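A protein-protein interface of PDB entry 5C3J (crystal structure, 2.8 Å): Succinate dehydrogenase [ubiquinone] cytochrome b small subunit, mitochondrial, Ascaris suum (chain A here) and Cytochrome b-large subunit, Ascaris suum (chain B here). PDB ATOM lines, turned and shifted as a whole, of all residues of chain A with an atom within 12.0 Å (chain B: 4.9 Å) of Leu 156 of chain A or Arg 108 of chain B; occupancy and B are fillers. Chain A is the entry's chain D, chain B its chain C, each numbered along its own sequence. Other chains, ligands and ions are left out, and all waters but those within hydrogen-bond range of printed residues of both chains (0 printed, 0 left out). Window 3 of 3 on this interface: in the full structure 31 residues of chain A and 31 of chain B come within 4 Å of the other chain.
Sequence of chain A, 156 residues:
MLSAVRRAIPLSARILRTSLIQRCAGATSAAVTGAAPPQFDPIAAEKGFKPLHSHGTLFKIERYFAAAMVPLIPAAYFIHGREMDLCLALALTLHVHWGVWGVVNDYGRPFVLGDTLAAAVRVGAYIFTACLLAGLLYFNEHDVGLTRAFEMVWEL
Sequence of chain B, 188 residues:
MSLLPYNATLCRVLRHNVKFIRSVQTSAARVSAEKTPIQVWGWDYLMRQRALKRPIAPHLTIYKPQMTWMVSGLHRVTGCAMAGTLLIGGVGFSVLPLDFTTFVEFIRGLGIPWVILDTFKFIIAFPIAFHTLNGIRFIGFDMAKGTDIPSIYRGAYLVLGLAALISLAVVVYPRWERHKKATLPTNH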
ATOM      1  N   VAL A 144      18.373  -1.696 -17.009  1.00  0.00           N
ATOM      2  CA  VAL A 144      17.100  -2.275 -17.425  1.00  0.00           C
ATOM      3  C   VAL A 144      16.248  -2.758 -16.237  1.00  0.00           C
ATOM      4  O   VAL A 144      15.029  -2.578 -16.245  1.00  0.00           O
ATOM      5  CB  VAL A 144      17.323  -3.402 -18.452  1.00  0.00           C
ATOM      6  CG1 VAL A 144      18.091  -2.871 -19.658  1.00  0.00           C
ATOM      7  CG2 VAL A 144      18.065  -4.577 -17.829  1.00  0.00           C
ATOM      8  N   THR A 147      13.258  -7.750 -14.347  1.00  0.00           N
ATOM      9  CA  THR A 147      12.314  -8.354 -15.281  1.00  0.00           C
ATOM     10  C   THR A 147      12.775  -8.152 -16.726  1.00  0.00           C
ATOM     11  O   THR A 147      12.879  -9.116 -17.487  1.00  0.00           O
ATOM     12  CB  THR A 147      10.895  -7.802 -15.074  1.00  0.00           C
ATOM     13  OG1 THR A 147      10.933  -6.378 -15.041  1.00  0.00           O
ATOM     14  CG2 THR A 147      10.306  -8.297 -13.754  1.00  0.00           C
ATOM     15  N   ARG A 148      13.090  -6.911 -17.091  1.00  0.00           N
ATOM     16  CA  ARG A 148      13.574  -6.614 -18.441  1.00  0.00           C
ATOM     17  C   ARG A 148      14.863  -7.382 -18.770  1.00  0.00           C
ATOM     18  O   ARG A 148      15.010  -7.889 -19.885  1.00  0.00           O
ATOM     19  CB  ARG A 148      13.796  -5.107 -18.626  1.00  0.00           C
ATOM     20  CG  ARG A 148      14.111  -4.666 -20.067  1.00  0.00           C
ATOM     21  CD  ARG A 148      12.873  -4.559 -20.963  1.00  0.00           C
ATOM     22  NE  ARG A 148      12.849  -5.552 -22.040  1.00  0.00           N
ATOM     23  CZ  ARG A 148      13.610  -5.503 -23.135  1.00  0.00           C
ATOM     24  NH1 ARG A 148      14.487  -4.518 -23.311  1.00  0.00           N
ATOM     25  NH2 ARG A 148      13.510  -6.458 -24.057  1.00  0.00           N
ATOM     26  N   ALA A 149      15.785  -7.461 -17.804  1.00  0.00           N
ATOM     27  CA  ALA A 149      17.080  -8.152 -17.993  1.00  0.00           C
ATOM     28  C   ALA A 149      16.859  -9.582 -18.429  1.00  0.00           C
ATOM     29  O   ALA A 149      17.508 -10.055 -19.372  1.00  0.00           O
ATOM     30  CB  ALA A 149      17.913  -8.121 -16.720  1.00  0.00           C
ATOM     31  N   PHE A 150      15.933 -10.260 -17.746  1.00  0.00           N
ATOM     32  CA  PHE A 150      15.507 -11.595 -18.164  1.00  0.00           C
ATOM     33  C   PHE A 150      14.922 -11.616 -19.591  1.00  0.00           C
ATOM     34  O   PHE A 150      15.328 -12.446 -20.408  1.00  0.00           O
ATOM     35  CB  PHE A 150      14.518 -12.206 -17.162  1.00  0.00           C
ATOM     36  CG  PHE A 150      15.169 -12.776 -15.927  1.00  0.00           C
ATOM     37  CD1 PHE A 150      14.976 -12.183 -14.681  1.00  0.00           C
ATOM     38  CD2 PHE A 150      15.975 -13.909 -16.013  1.00  0.00           C
ATOM     39  CE1 PHE A 150      15.581 -12.703 -13.551  1.00  0.00           C
ATOM     40  CE2 PHE A 150      16.580 -14.432 -14.884  1.00  0.00           C
ATOM     41  CZ  PHE A 150      16.383 -13.826 -13.654  1.00  0.00           C
ATOM     42  N   GLU A 151      13.988 -10.714 -19.897  1.00  0.00           N
ATOM     43  CA  GLU A 151      13.429 -10.632 -21.255  1.00  0.00           C
ATOM     44  C   GLU A 151      14.511 -10.658 -22.335  1.00  0.00           C
ATOM     45  O   GLU A 151      14.391 -11.384 -23.319  1.00  0.00           O
ATOM     46  CB  GLU A 151      12.604  -9.353 -21.459  1.00  0.00           C
ATOM     47  CG  GLU A 151      11.241  -9.315 -20.787  1.00  0.00           C
ATOM     48  CD  GLU A 151      10.364  -8.200 -21.338  1.00  0.00           C
ATOM     49  OE1 GLU A 151      10.214  -7.163 -20.647  1.00  0.00           O
ATOM     50  OE2 GLU A 151       9.832  -8.362 -22.462  1.00  0.00           O
ATOM     51  N   MET A 152      15.558  -9.857 -22.142  1.00  0.00           N
ATOM     52  CA  MET A 152      16.553  -9.594 -23.192  1.00  0.00           C
ATOM     53  C   MET A 152      17.486 -10.772 -23.490  1.00  0.00           C
ATOM     54  O   MET A 152      17.943 -10.936 -24.625  1.00  0.00           O
ATOM     55  CB  MET A 152      17.371  -8.346 -22.840  1.00  0.00           C
ATOM     56  CG  MET A 152      16.536  -7.075 -22.839  1.00  0.00           C
ATOM     57  SD  MET A 152      17.375  -5.638 -22.150  1.00  0.00           S
ATOM     58  CE  MET A 152      18.730  -5.478 -23.317  1.00  0.00           C
ATOM     59  N   VAL A 153      17.787 -11.571 -22.470  1.00  0.00           N
ATOM     60  CA  VAL A 153      18.558 -12.793 -22.674  1.00  0.00           C
ATOM     61  C   VAL A 153      17.646 -13.834 -23.310  1.00  0.00           C
ATOM     62  O   VAL A 153      18.081 -14.630 -24.147  1.00  0.00           O
ATOM     63  CB  VAL A 153      19.187 -13.334 -21.364  1.00  0.00           C
ATOM     64  CG1 VAL A 153      20.278 -12.398 -20.865  1.00  0.00           C
ATOM     65  CG2 VAL A 153      18.143 -13.542 -20.274  1.00  0.00           C
ATOM     66  N   TRP A 154      16.373 -13.796 -22.929  1.00  0.00           N
ATOM     67  CA  TRP A 154      15.383 -14.739 -23.439  1.00  0.00           C
ATOM     68  C   TRP A 154      15.099 -14.474 -24.930  1.00  0.00           C
ATOM     69  O   TRP A 154      14.964 -15.415 -25.714  1.00  0.00           O
ATOM     70  CB  TRP A 154      14.089 -14.686 -22.592  1.00  0.00           C
ATOM     71  CG  TRP A 154      13.679 -16.037 -22.044  1.00  0.00           C
ATOM     72  CD1 TRP A 154      12.681 -16.842 -22.505  1.00  0.00           C
ATOM     73  CD2 TRP A 154      14.284 -16.739 -20.947  1.00  0.00           C
ATOM     74  NE1 TRP A 154      12.624 -18.000 -21.766  1.00  0.00           N
ATOM     75  CE2 TRP A 154      13.596 -17.961 -20.802  1.00  0.00           C
ATOM     76  CE3 TRP A 154      15.343 -16.453 -20.075  1.00  0.00           C
ATOM     77  CZ2 TRP A 154      13.928 -18.896 -19.818  1.00  0.00           C
ATOM     78  CZ3 TRP A 154      15.675 -17.386 -19.098  1.00  0.00           C
ATOM     79  CH2 TRP A 154      14.966 -18.591 -18.977  1.00  0.00           C
ATOM     80  N   GLU A 155      15.037 -13.194 -25.304  1.00  0.00           N
ATOM     81  CA  GLU A 155      14.848 -12.756 -26.698  1.00  0.00           C
ATOM     82  C   GLU A 155      15.948 -13.200 -27.653  1.00  0.00           C
ATOM     83  O   GLU A 155      15.719 -13.240 -28.861  1.00  0.00           O
ATOM     84  CB  GLU A 155      14.755 -11.229 -26.776  1.00  0.00           C
ATOM     85  CG  GLU A 155      13.374 -10.651 -26.498  1.00  0.00           C
ATOM     86  CD  GLU A 155      13.413  -9.151 -26.258  1.00  0.00           C
ATOM     87  OE1 GLU A 155      14.451  -8.523 -26.546  1.00  0.00           O
ATOM     88  OE2 GLU A 155      12.408  -8.599 -25.772  1.00  0.00           O
ATOM     89  N   LEU A 156      17.138 -13.497 -27.135  1.00  0.00           N
ATOM     90  CA  LEU A 156      18.236 -13.994 -27.969  1.00  0.00           C
ATOM     91  C   LEU A 156      17.868 -15.327 -28.624  1.00  0.00           C
ATOM     92  O   LEU A 156      18.664 -15.907 -29.367  1.00  0.00           O
ATOM     93  CB  LEU A 156      19.514 -14.187 -27.142  1.00  0.00           C
ATOM     94  CG  LEU A 156      20.199 -12.974 -26.500  1.00  0.00           C
ATOM     95  CD1 LEU A 156      21.097 -13.437 -25.364  1.00  0.00           C
ATOM     96  CD2 LEU A 156      21.007 -12.170 -27.508  1.00  0.00           C
ATOM     97  OXT LEU A 156      16.774 -15.872 -28.421  1.00  0.00           O
ATOM     98  N   VAL B 104      24.314  -7.788 -23.675  1.00  0.00           N
ATOM     99  CA  VAL B 104      23.434  -8.651 -24.466  1.00  0.00           C
ATOM    100  C   VAL B 104      23.823  -8.607 -25.952  1.00  0.00           C
ATOM    101  O   VAL B 104      23.936  -9.657 -26.604  1.00  0.00           O
ATOM    102  CB  VAL B 104      21.948  -8.275 -24.279  1.00  0.00           C
ATOM    103  CG1 VAL B 104      21.056  -9.105 -25.191  1.00  0.00           C
ATOM    104  CG2 VAL B 104      21.529  -8.486 -22.833  1.00  0.00           C
ATOM    105  N   GLU B 105      24.030  -7.396 -26.473  1.00  0.00           N
ATOM    106  CA  GLU B 105      24.455  -7.209 -27.871  1.00  0.00           C
ATOM    107  C   GLU B 105      25.806  -7.877 -28.136  1.00  0.00           C
ATOM    108  O   GLU B 105      26.010  -8.494 -29.189  1.00  0.00           O
ATOM    109  CB  GLU B 105      24.512  -5.717 -28.255  1.00  0.00           C
ATOM    110  CG  GLU B 105      23.295  -5.201 -29.023  1.00  0.00           C
ATOM    111  CD  GLU B 105      22.097  -4.901 -28.133  1.00  0.00           C
ATOM    112  OE1 GLU B 105      21.576  -5.837 -27.482  1.00  0.00           O
ATOM    113  OE2 GLU B 105      21.664  -3.725 -28.097  1.00  0.00           O
ATOM    114  N   PHE B 106      26.721  -7.754 -27.177  1.00  0.00           N
ATOM    115  CA  PHE B 106      28.006  -8.434 -27.262  1.00  0.00           C
ATOM    116  C   PHE B 106      27.789  -9.911 -27.606  1.00  0.00           C
ATOM    117  O   PHE B 106      28.310 -10.385 -28.621  1.00  0.00           O
ATOM    118  CB  PHE B 106      28.802  -8.257 -25.958  1.00  0.00           C
ATOM    119  CG  PHE B 106      30.045  -9.111 -25.864  1.00  0.00           C
ATOM    120  CD1 PHE B 106      30.864  -9.325 -26.972  1.00  0.00           C
ATOM    121  CD2 PHE B 106      30.414  -9.681 -24.645  1.00  0.00           C
ATOM    122  CE1 PHE B 106      32.003 -10.109 -26.870  1.00  0.00           C
ATOM    123  CE2 PHE B 106      31.557 -10.459 -24.538  1.00  0.00           C
ATOM    124  CZ  PHE B 106      32.352 -10.675 -25.653  1.00  0.00           C
ATOM    125  N   ILE B 107      26.984 -10.615 -26.803  1.00  0.00           N
ATOM    126  CA  ILE B 107      26.831 -12.075 -26.972  1.00  0.00           C
ATOM    127  C   ILE B 107      26.045 -12.423 -28.247  1.00  0.00           C
ATOM    128  O   ILE B 107      26.297 -13.462 -28.864  1.00  0.00           O
ATOM    129  CB  ILE B 107      26.270 -12.822 -25.707  1.00  0.00           C
ATOM    130  CG1 ILE B 107      24.744 -12.981 -25.744  1.00  0.00           C
ATOM    131  CG2 ILE B 107      26.730 -12.184 -24.398  1.00  0.00           C
ATOM    132  CD1 ILE B 107      24.272 -14.253 -26.434  1.00  0.00           C
ATOM    133  N   ARG B 108      25.098 -11.563 -28.634  1.00  0.00           N
ATOM    134  CA  ARG B 108      24.377 -11.730 -29.903  1.00  0.00           C
ATOM    135  C   ARG B 108      25.341 -11.573 -31.083  1.00  0.00           C
ATOM    136  O   ARG B 108      25.312 -12.357 -32.035  1.00  0.00           O
ATOM    137  CB  ARG B 108      23.221 -10.734 -30.014  1.00  0.00           C
ATOM    138  CG  ARG B 108      22.517 -10.733 -31.371  1.00  0.00           C
ATOM    139  CD  ARG B 108      21.037 -10.392 -31.258  1.00  0.00           C
ATOM    140  NE  ARG B 108      20.794  -9.288 -30.326  1.00  0.00           N
ATOM    141  CZ  ARG B 108      19.595  -8.925 -29.876  1.00  0.00           C
ATOM    142  NH1 ARG B 108      19.499  -7.906 -29.025  1.00  0.00           N
ATOM    143  NH2 ARG B 108      18.494  -9.563 -30.273  1.00  0.00           N
ATOM    144  N   GLY B 109      26.209 -10.567 -30.995  1.00  0.00           N
ATOM    145  CA  GLY B 109      27.285 -10.384 -31.962  1.00  0.00           C
ATOM    146  C   GLY B 109      28.169 -11.608 -32.173  1.00  0.00           C
ATOM    147  O   GLY B 109      28.834 -11.713 -33.204  1.00  0.00           O
ATOM    148  N   LEU B 110      28.179 -12.535 -31.213  1.00  0.00           N
ATOM    149  CA  LEU B 110      29.009 -13.739 -31.317  1.00  0.00           C
ATOM    150  C   LEU B 110      28.449 -14.782 -32.290  1.00  0.00           C
ATOM    151  O   LEU B 110      29.180 -15.678 -32.713  1.00  0.00           O
ATOM    152  CB  LEU B 110      29.221 -14.378 -29.939  1.00  0.00           C
ATOM    153  CG  LEU B 110      29.731 -13.466 -28.818  1.00  0.00           C
ATOM    154  CD1 LEU B 110      29.893 -14.243 -27.519  1.00  0.00           C
ATOM    155  CD2 LEU B 110      31.035 -12.785 -29.209  1.00  0.00           C
ATOM    156  N   GLY B 111      27.165 -14.677 -32.632  1.00  0.00           N
ATOM    157  CA  GLY B 111      26.544 -15.576 -33.617  1.00  0.00           C
ATOM    158  C   GLY B 111      26.476 -17.027 -33.169  1.00  0.00           C
ATOM    159  O   GLY B 111      26.837 -17.926 -33.916  1.00  0.00           O
ATOM    160  N   LEU B 117      22.082 -21.549 -27.266  1.00  0.00           N
ATOM    161  CA  LEU B 117      21.482 -20.403 -26.580  1.00  0.00           C
ATOM    162  C   LEU B 117      20.269 -20.816 -25.762  1.00  0.00           C
ATOM    163  O   LEU B 117      20.088 -20.339 -24.645  1.00  0.00           O
ATOM    164  CB  LEU B 117      21.096 -19.301 -27.572  1.00  0.00           C
ATOM    165  CG  LEU B 117      22.268 -18.461 -28.084  1.00  0.00           C
ATOM    166  CD1 LEU B 117      21.882 -17.692 -29.341  1.00  0.00           C
ATOM    167  CD2 LEU B 117      22.764 -17.520 -26.994  1.00  0.00           C
ATOM    168  N   LYS B 121      19.699 -21.067 -21.658  1.00  0.00           N
ATOM    169  CA  LYS B 121      18.416 -20.594 -21.118  1.00  0.00           C
ATOM    170  C   LYS B 121      17.752 -21.628 -20.213  1.00  0.00           C
ATOM    171  O   LYS B 121      17.195 -21.285 -19.169  1.00  0.00           O
ATOM    172  CB  LYS B 121      17.442 -20.235 -22.249  1.00  0.00           C
ATOM    173  CG  LYS B 121      17.729 -18.926 -22.969  1.00  0.00           C
ATOM    174  CD  LYS B 121      16.820 -18.747 -24.183  1.00  0.00           C
ATOM    175  CE  LYS B 121      17.427 -17.834 -25.242  1.00  0.00           C
ATOM    176  NZ  LYS B 121      17.037 -18.267 -26.612  1.00  0.00           N
ATOM    177  N   ARG B 175      10.615 -19.994 -28.396  1.00  0.00           N
ATOM    178  CA  ARG B 175      11.379 -20.328 -29.596  1.00  0.00           C
ATOM    179  C   ARG B 175      10.513 -21.044 -30.649  1.00  0.00           C
ATOM    180  O   ARG B 175      10.707 -20.846 -31.844  1.00  0.00           O
ATOM    181  CB  ARG B 175      12.622 -21.164 -29.242  1.00  0.00           C
ATOM    182  CG  ARG B 175      13.492 -21.607 -30.424  1.00  0.00           C
ATOM    183  CD  ARG B 175      13.808 -20.514 -31.449  1.00  0.00           C
ATOM    184  NE  ARG B 175      15.152 -19.941 -31.320  1.00  0.00           N
ATOM    185  CZ  ARG B 175      15.525 -19.059 -30.393  1.00  0.00           C
ATOM    186  NH1 ARG B 175      16.773 -18.597 -30.377  1.00  0.00           N
ATOM    187  NH2 ARG B 175      14.669 -18.637 -29.468  1.00  0.00           N
ATOM    188  N   ARG B 178       8.350 -18.373 -31.953  1.00  0.00           N
ATOM    189  CA  ARG B 178       9.121 -17.429 -32.771  1.00  0.00           C
ATOM    190  C   ARG B 178       9.275 -17.965 -34.199  1.00  0.00           C
ATOM    191  O   ARG B 178       9.046 -17.244 -35.164  1.00  0.00           O
ATOM    192  CB  ARG B 178      10.504 -17.153 -32.161  1.00  0.00           C
ATOM    193  CG  ARG B 178      10.565 -15.953 -31.216  1.00  0.00           C
ATOM    194  CD  ARG B 178      11.811 -15.118 -31.477  1.00  0.00           C
ATOM    195  NE  ARG B 178      12.982 -15.513 -30.684  1.00  0.00           N
ATOM    196  CZ  ARG B 178      14.238 -15.574 -31.137  1.00  0.00           C
ATOM    197  NH1 ARG B 178      14.534 -15.322 -32.408  1.00  0.00           N
ATOM    198  NH2 ARG B 178      15.214 -15.917 -30.314  1.00  0.00           N
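Ala 149 of chain A touches none of the printed residues of chain B.
Of the printed residues of chain B, Met 152 of chain A touches Val 104 (3.7 Å).
Val 104 of chain B touches two residues of chain A.
No residue of chain A comes within 4 Å of Glu 105 of chain B.
No residue of chain A comes within 4 Å of Leu 110 of chain B.
No residue of chain A comes within 4 Å of Gly 111 of chain B.
Of chain A, only Leu 156 comes within 4 Å of Leu 117 of chain B.
Printed residues of chain A within 4 Å of Lys 121 of chain B: Val 153, Trp 154 and Leu 156.
Printed residues of chain A within 4 Å of Arg 175 of chain B: Leu 156 (3.4 Å).
The nearest residue of chain A that does not touch Arg 108 of chain B is Glu 155 of chain A (4.8 Å).
The nearest printed residue of chain A that does not touch Arg 178 of chain B is Trp 154 of chain A (4.6 Å).
Of the 11 printed residues of chain A, 5 touch a printed residue of chain B.
Hydrophobic or aromatic side chains of chain A that line the printed part of chain B: Trp 154 and Leu 156.
Among the printed residues, no Asp or Glu carboxylate lies within 4 Å of a Lys or Arg side-chain nitrogen of the other chain.
The side-chain carboxylate (OE1) of Glu 105 of chain B lies within salt-bridge range of the guanidinium group (NH1) of Arg 108 of chain B (3.3 Å).
The guanidinium group of Arg 148 of chain A lies within hydrogen-bond range of the side-chain sulfur of Met 152 of chain A.
The side-chain carboxylate (OE2) of Glu 155 of chain A lies within salt-bridge range of the guanidinium group (NH2) of Arg 148 of chain A (3.0 Å).
Among the printed residues, merely in contact across the chains: Leu 156 of chain A with Ile 107 of chain B (3.4 Å), Val 153 of chain A with Lys 121 of chain B (3.4 Å), Trp 154 of chain A with Lys 121 of chain B (3.5 Å), Leu 156 of chain A with Arg 108 of chain B (3.6 Å), Met 152 of chain A with Val 104 of chain B (3.7 Å), Leu 156 of chain A with Leu 117 of chain B (3.7 Å) and Leu 156 of chain A with Val 104 of chain B (3.8 Å).
The side-chain amino group (NZ) of Lys 121 of chain B is in salt-bridge range of the chain-end carboxylate (OXT) of Leu 156 of chain A, 3.0 Å away.
The guanidinium group (NH1) of Arg 175 of chain B is in salt-bridge range of the chain-end carboxylate (OXT) of Leu 156 of chain A (3.4 Å).
NH2 of Arg 178 of chain B is in hydrogen-bond range of O of Glu 155 of chain A, at 3.1 Å.
NH2 of Arg 178 of chain B is in salt-bridge range of OXT of Leu 156 of chain A (2.5 Å).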
